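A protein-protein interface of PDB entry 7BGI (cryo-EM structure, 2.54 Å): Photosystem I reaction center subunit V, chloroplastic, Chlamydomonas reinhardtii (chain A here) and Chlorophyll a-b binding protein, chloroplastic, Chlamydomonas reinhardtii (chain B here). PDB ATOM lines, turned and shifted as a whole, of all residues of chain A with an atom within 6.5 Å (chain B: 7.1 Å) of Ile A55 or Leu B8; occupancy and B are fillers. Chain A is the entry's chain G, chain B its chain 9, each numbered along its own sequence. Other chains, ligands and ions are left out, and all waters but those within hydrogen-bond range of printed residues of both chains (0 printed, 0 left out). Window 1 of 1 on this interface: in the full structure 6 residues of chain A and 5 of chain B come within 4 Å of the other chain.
The side-chain hydroxyl (OG1) of Thr B3 lies within hydrogen-bond range of the backbone carbonyl oxygen (O) of Leu B8 (3.0 Å).
OG1 of Thr A54 touches O of Asp B25, at 3.9 Å. CD1 of Leu B8 touches O of Ile A55 (3.8 Å). CD1 of Leu B8 touches CA of Phe A56 (3.8 Å). Gly B7 touches Ala A57. Ala A57 touches Leu B8 (O to CB, 3.7 Å). OD1 of Asn A59 touches CA of Gly B7, 3.8 Å away.
Of chain B, only Leu B8 comes within 4 Å of Ile A55. Printed residues of chain B within 4 Å of Ala A57: Gly B7 and Leu B8. Printed residues of chain B within 4 Å of Asn A59: Gly B7 (3.8 Å). Trp B4 touches none of the printed residues of chain A. Pro B11 touches none of the printed residues of chain A.
Of the 8 printed residues of chain A, 5 touch a printed residue of chain B. Hydrophobic or aromatic side chains of chain A within 4 Å of the printed part of chain B: Ala A57. Hydrophobic or aromatic side chains of chain B within 4 Å of the printed part of chain A: Leu B8. Among the printed residues, no Asp or Glu carboxylate lies within 4 Å of a Lys or Arg side-chain nitrogen of the other chain.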
ATOM      1  N   SER A  53      16.304  39.834  23.216  1.00  0.00           N
ATOM      2  CA  SER A  53      16.508  39.026  22.020  1.00  0.00           C
ATOM      3  C   SER A  53      15.688  37.750  22.126  1.00  0.00           C
ATOM      4  O   SER A  53      15.264  37.348  23.212  1.00  0.00           O
ATOM      5  CB  SER A  53      17.988  38.687  21.811  1.00  0.00           C
ATOM      6  OG  SER A  53      18.691  39.785  21.261  1.00  0.00           O
ATOM      7  N   THR A  54      15.477  37.117  20.974  1.00  0.00           N
ATOM      8  CA  THR A  54      14.736  35.867  20.872  1.00  0.00           C
ATOM      9  C   THR A  54      15.666  34.814  20.289  1.00  0.00           C
ATOM     10  O   THR A  54      16.280  35.037  19.240  1.00  0.00           O
ATOM     11  CB  THR A  54      13.487  36.018  20.000  1.00  0.00           C
ATOM     12  OG1 THR A  54      12.678  37.089  20.499  1.00  0.00           O
ATOM     13  CG2 THR A  54      12.670  34.734  20.010  1.00  0.00           C
ATOM     14  N   ILE A  55      15.776  33.678  20.966  1.00  0.00           N
ATOM     15  CA  ILE A  55      16.646  32.597  20.518  1.00  0.00           C
ATOM     16  C   ILE A  55      15.877  31.741  19.521  1.00  0.00           C
ATOM     17  O   ILE A  55      14.917  31.055  19.882  1.00  0.00           O
ATOM     18  CB  ILE A  55      17.157  31.760  21.696  1.00  0.00           C
ATOM     19  CG1 ILE A  55      18.054  32.611  22.596  1.00  0.00           C
ATOM     20  CG2 ILE A  55      17.917  30.542  21.193  1.00  0.00           C
ATOM     21  CD1 ILE A  55      19.288  33.150  21.896  1.00  0.00           C
ATOM     22  N   PHE A  56      16.301  31.784  18.260  1.00  0.00           N
ATOM     23  CA  PHE A  56      15.675  31.000  17.197  1.00  0.00           C
ATOM     24  C   PHE A  56      16.385  29.654  17.070  1.00  0.00           C
ATOM     25  O   PHE A  56      17.061  29.360  16.087  1.00  0.00           O
ATOM     26  CB  PHE A  56      15.697  31.770  15.882  1.00  0.00           C
ATOM     27  CG  PHE A  56      14.813  32.978  15.875  1.00  0.00           C
ATOM     28  CD1 PHE A  56      13.478  32.872  15.533  1.00  0.00           C
ATOM     29  CD2 PHE A  56      15.317  34.221  16.215  1.00  0.00           C
ATOM     30  CE1 PHE A  56      12.661  33.984  15.529  1.00  0.00           C
ATOM     31  CE2 PHE A  56      14.506  35.335  16.214  1.00  0.00           C
ATOM     32  CZ  PHE A  56      13.177  35.216  15.869  1.00  0.00           C
ATOM     33  N   ALA A  57      16.224  28.840  18.110  1.00  0.00           N
ATOM     34  CA  ALA A  57      16.845  27.525  18.141  1.00  0.00           C
ATOM     35  C   ALA A  57      16.225  26.612  17.093  1.00  0.00           C
ATOM     36  O   ALA A  57      15.004  26.565  16.927  1.00  0.00           O
ATOM     37  CB  ALA A  57      16.701  26.905  19.530  1.00  0.00           C
ATOM     38  N   THR A  58      17.079  25.886  16.381  1.00  0.00           N
ATOM     39  CA  THR A  58      16.642  24.969  15.344  1.00  0.00           C
ATOM     40  C   THR A  58      17.344  23.634  15.520  1.00  0.00           C
ATOM     41  O   THR A  58      18.390  23.536  16.166  1.00  0.00           O
ATOM     42  CB  THR A  58      16.923  25.514  13.935  1.00  0.00           C
ATOM     43  OG1 THR A  58      18.281  25.961  13.850  1.00  0.00           O
ATOM     44  CG2 THR A  58      15.981  26.664  13.611  1.00  0.00           C
ATOM     45  N   ASN A  59      16.751  22.603  14.931  1.00  0.00           N
ATOM     46  CA  ASN A  59      17.307  21.261  15.005  1.00  0.00           C
ATOM     47  C   ASN A  59      18.363  21.006  13.942  1.00  0.00           C
ATOM     48  O   ASN A  59      18.821  19.865  13.816  1.00  0.00           O
ATOM     49  CB  ASN A  59      16.193  20.224  14.892  1.00  0.00           C
ATOM     50  CG  ASN A  59      15.312  20.191  16.115  1.00  0.00           C
ATOM     51  OD1 ASN A  59      15.758  20.485  17.222  1.00  0.00           O
ATOM     52  ND2 ASN A  59      14.050  19.829  15.924  1.00  0.00           N
ATOM     53  N   ILE A  66      16.150  29.885  10.954  1.00  0.00           N
ATOM     54  CA  ILE A  66      15.176  30.506  10.058  1.00  0.00           C
ATOM     55  C   ILE A  66      15.649  31.881   9.586  1.00  0.00           C
ATOM     56  O   ILE A  66      15.385  32.278   8.442  1.00  0.00           O
ATOM     57  CB  ILE A  66      13.798  30.556  10.754  1.00  0.00           C
ATOM     58  CG1 ILE A  66      12.727  31.177   9.857  1.00  0.00           C
ATOM     59  CG2 ILE A  66      13.870  31.269  12.102  1.00  0.00           C
ATOM     60  CD1 ILE A  66      12.280  30.277   8.731  1.00  0.00           C
ATOM     61  N   ARG B   1       3.931  21.656  26.028  1.00  0.00           N
ATOM     62  CA  ARG B   1       3.273  22.700  25.252  1.00  0.00           C
ATOM     63  C   ARG B   1       3.959  22.876  23.900  1.00  0.00           C
ATOM     64  O   ARG B   1       5.112  23.297  23.838  1.00  0.00           O
ATOM     65  CB  ARG B   1       3.270  24.019  26.026  1.00  0.00           C
ATOM     66  CG  ARG B   1       2.262  25.039  25.527  1.00  0.00           C
ATOM     67  CD  ARG B   1       2.934  26.110  24.690  1.00  0.00           C
ATOM     68  NE  ARG B   1       4.020  26.764  25.411  1.00  0.00           N
ATOM     69  CZ  ARG B   1       3.882  27.875  26.119  1.00  0.00           C
ATOM     70  NH1 ARG B   1       2.716  28.488  26.221  1.00  0.00           N
ATOM     71  NH2 ARG B   1       4.941  28.386  26.737  1.00  0.00           N
ATOM     72  N   PRO B   2       3.252  22.550  22.820  1.00  0.00           N
ATOM     73  CA  PRO B   2       3.842  22.689  21.486  1.00  0.00           C
ATOM     74  C   PRO B   2       3.944  24.144  21.061  1.00  0.00           C
ATOM     75  O   PRO B   2       3.036  24.950  21.284  1.00  0.00           O
ATOM     76  CB  PRO B   2       2.873  21.915  20.588  1.00  0.00           C
ATOM     77  CG  PRO B   2       1.567  22.007  21.292  1.00  0.00           C
ATOM     78  CD  PRO B   2       1.873  22.034  22.766  1.00  0.00           C
ATOM     79  N   THR B   3       5.068  24.476  20.438  1.00  0.00           N
ATOM     80  CA  THR B   3       5.338  25.821  19.961  1.00  0.00           C
ATOM     81  C   THR B   3       5.169  25.878  18.447  1.00  0.00           C
ATOM     82  O   THR B   3       4.944  24.863  17.782  1.00  0.00           O
ATOM     83  CB  THR B   3       6.740  26.276  20.372  1.00  0.00           C
ATOM     84  OG1 THR B   3       7.711  25.354  19.865  1.00  0.00           O
ATOM     85  CG2 THR B   3       6.853  26.344  21.884  1.00  0.00           C
ATOM     86  N   TRP B   4       5.277  27.090  17.904  1.00  0.00           N
ATOM     87  CA  TRP B   4       5.135  27.286  16.468  1.00  0.00           C
ATOM     88  C   TRP B   4       6.302  26.717  15.673  1.00  0.00           C
ATOM     89  O   TRP B   4       6.082  26.150  14.604  1.00  0.00           O
ATOM     90  CB  TRP B   4       4.960  28.774  16.150  1.00  0.00           C
ATOM     91  CG  TRP B   4       6.141  29.629  16.489  1.00  0.00           C
ATOM     92  CD1 TRP B   4       6.546  30.008  17.731  1.00  0.00           C
ATOM     93  CD2 TRP B   4       7.070  30.214  15.571  1.00  0.00           C
ATOM     94  NE1 TRP B   4       7.666  30.794  17.648  1.00  0.00           N
ATOM     95  CE2 TRP B   4       8.009  30.935  16.330  1.00  0.00           C
ATOM     96  CE3 TRP B   4       7.199  30.199  14.181  1.00  0.00           C
ATOM     97  CZ2 TRP B   4       9.062  31.632  15.748  1.00  0.00           C
ATOM     98  CZ3 TRP B   4       8.244  30.889  13.606  1.00  0.00           C
ATOM     99  CH2 TRP B   4       9.161  31.598  14.386  1.00  0.00           C
ATOM    100  N   LEU B   5       7.532  26.840  16.159  1.00  0.00           N
ATOM    101  CA  LEU B   5       8.693  26.322  15.445  1.00  0.00           C
ATOM    102  C   LEU B   5       9.183  25.075  16.167  1.00  0.00           C
ATOM    103  O   LEU B   5       9.395  25.121  17.397  1.00  0.00           O
ATOM    104  CB  LEU B   5       9.795  27.378  15.344  1.00  0.00           C
ATOM    105  CG  LEU B   5      10.663  27.325  14.086  1.00  0.00           C
ATOM    106  CD1 LEU B   5       9.808  27.215  12.832  1.00  0.00           C
ATOM    107  CD2 LEU B   5      11.563  28.546  14.015  1.00  0.00           C
ATOM    108  N   PRO B   6       9.358  23.951  15.472  1.00  0.00           N
ATOM    109  CA  PRO B   6       9.839  22.737  16.143  1.00  0.00           C
ATOM    110  C   PRO B   6      11.267  22.916  16.637  1.00  0.00           C
ATOM    111  O   PRO B   6      12.121  23.471  15.943  1.00  0.00           O
ATOM    112  CB  PRO B   6       9.747  21.666  15.051  1.00  0.00           C
ATOM    113  CG  PRO B   6       8.774  22.206  14.060  1.00  0.00           C
ATOM    114  CD  PRO B   6       8.963  23.692  14.079  1.00  0.00           C
ATOM    115  N   GLY B   7      11.516  22.446  17.855  1.00  0.00           N
ATOM    116  CA  GLY B   7      12.827  22.568  18.450  1.00  0.00           C
ATOM    117  C   GLY B   7      13.131  23.933  19.017  1.00  0.00           C
ATOM    118  O   GLY B   7      14.255  24.163  19.477  1.00  0.00           O
ATOM    119  N   LEU B   8      12.164  24.845  19.000  1.00  0.00           N
ATOM    120  CA  LEU B   8      12.324  26.200  19.509  1.00  0.00           C
ATOM    121  C   LEU B   8      11.654  26.290  20.872  1.00  0.00           C
ATOM    122  O   LEU B   8      10.467  25.975  21.006  1.00  0.00           O
ATOM    123  CB  LEU B   8      11.719  27.217  18.541  1.00  0.00           C
ATOM    124  CG  LEU B   8      11.786  28.707  18.890  1.00  0.00           C
ATOM    125  CD1 LEU B   8      12.225  29.507  17.678  1.00  0.00           C
ATOM    126  CD2 LEU B   8      10.443  29.211  19.395  1.00  0.00           C
ATOM    127  N   ASN B   9      12.407  26.715  21.868  1.00  0.00           N
ATOM    128  CA  ASN B   9      11.838  26.842  23.199  1.00  0.00           C
ATOM    129  C   ASN B   9      10.989  28.108  23.281  1.00  0.00           C
ATOM    130  O   ASN B   9      11.337  29.124  22.672  1.00  0.00           O
ATOM    131  CB  ASN B   9      12.941  26.888  24.251  1.00  0.00           C
ATOM    132  CG  ASN B   9      14.056  25.908  23.964  1.00  0.00           C
ATOM    133  OD1 ASN B   9      15.130  26.292  23.502  1.00  0.00           O
ATOM    134  ND2 ASN B   9      13.804  24.633  24.231  1.00  0.00           N
ATOM    135  N   PRO B  10       9.875  28.070  24.010  1.00  0.00           N
ATOM    136  CA  PRO B  10       9.043  29.262  24.125  1.00  0.00           C
ATOM    137  C   PRO B  10       9.762  30.334  24.918  1.00  0.00           C
ATOM    138  O   PRO B  10      10.631  30.032  25.757  1.00  0.00           O
ATOM    139  CB  PRO B  10       7.796  28.752  24.862  1.00  0.00           C
ATOM    140  CG  PRO B  10       8.236  27.517  25.555  1.00  0.00           C
ATOM    141  CD  PRO B  10       9.277  26.905  24.681  1.00  0.00           C
ATOM    142  N   PRO B  11       9.446  31.604  24.675  1.00  0.00           N
ATOM    143  CA  PRO B  11      10.123  32.684  25.398  1.00  0.00           C
ATOM    144  C   PRO B  11       9.741  32.721  26.870  1.00  0.00           C
ATOM    145  O   PRO B  11       8.765  32.111  27.311  1.00  0.00           O
ATOM    146  CB  PRO B  11       9.650  33.951  24.675  1.00  0.00           C
ATOM    147  CG  PRO B  11       9.060  33.482  23.384  1.00  0.00           C
ATOM    148  CD  PRO B  11       8.520  32.123  23.657  1.00  0.00           C
ATOM    149  N   ASN B  22       0.992  29.893  22.349  1.00  0.00           N
ATOM    150  CA  ASN B  22       1.746  28.884  21.621  1.00  0.00           C
ATOM    151  C   ASN B  22       3.216  29.262  21.522  1.00  0.00           C
ATOM    152  O   ASN B  22       3.949  28.691  20.711  1.00  0.00           O
ATOM    153  CB  ASN B  22       1.153  28.672  20.229  1.00  0.00           C
ATOM    154  CG  ASN B  22      -0.169  27.941  20.268  1.00  0.00           C
ATOM    155  OD1 ASN B  22      -0.469  27.232  21.227  1.00  0.00           O
ATOM    156  ND2 ASN B  22      -0.970  28.108  19.224  1.00  0.00           N
ATOM    157  N   GLY B  23       3.652  30.221  22.337  1.00  0.00           N
ATOM    158  CA  GLY B  23       5.032  30.668  22.326  1.00  0.00           C
ATOM    159  C   GLY B  23       5.448  31.333  21.036  1.00  0.00           C
ATOM    160  O   GLY B  23       6.611  31.222  20.638  1.00  0.00           O
ATOM    161  N   PHE B  24       4.531  32.025  20.371  1.00  0.00           N
ATOM    162  CA  PHE B  24       4.819  32.695  19.108  1.00  0.00           C
ATOM    163  C   PHE B  24       4.954  34.193  19.340  1.00  0.00           C
ATOM    164  O   PHE B  24       3.955  34.898  19.503  1.00  0.00           O
ATOM    165  CB  PHE B  24       3.740  32.406  18.071  1.00  0.00           C
ATOM    166  CG  PHE B  24       3.858  33.246  16.833  1.00  0.00           C
ATOM    167  CD1 PHE B  24       4.918  33.070  15.963  1.00  0.00           C
ATOM    168  CD2 PHE B  24       2.924  34.226  16.549  1.00  0.00           C
ATOM    169  CE1 PHE B  24       5.036  33.844  14.827  1.00  0.00           C
ATOM    170  CE2 PHE B  24       3.039  35.004  15.418  1.00  0.00           C
ATOM    171  CZ  PHE B  24       4.096  34.812  14.556  1.00  0.00           C
ATOM    172  N   ASP B  25       6.191  34.669  19.346  1.00  0.00           N
ATOM    173  CA  ASP B  25       6.509  36.078  19.511  1.00  0.00           C
ATOM    174  C   ASP B  25       7.939  36.334  19.049  1.00  0.00           C
ATOM    175  O   ASP B  25       8.804  36.629  19.882  1.00  0.00           O
ATOM    176  CB  ASP B  25       6.336  36.521  20.963  1.00  0.00           C
ATOM    177  CG  ASP B  25       6.188  38.019  21.095  1.00  0.00           C
ATOM    178  OD1 ASP B  25       5.969  38.684  20.064  1.00  0.00           O
ATOM    179  OD2 ASP B  25       6.283  38.533  22.229  1.00  0.00           O
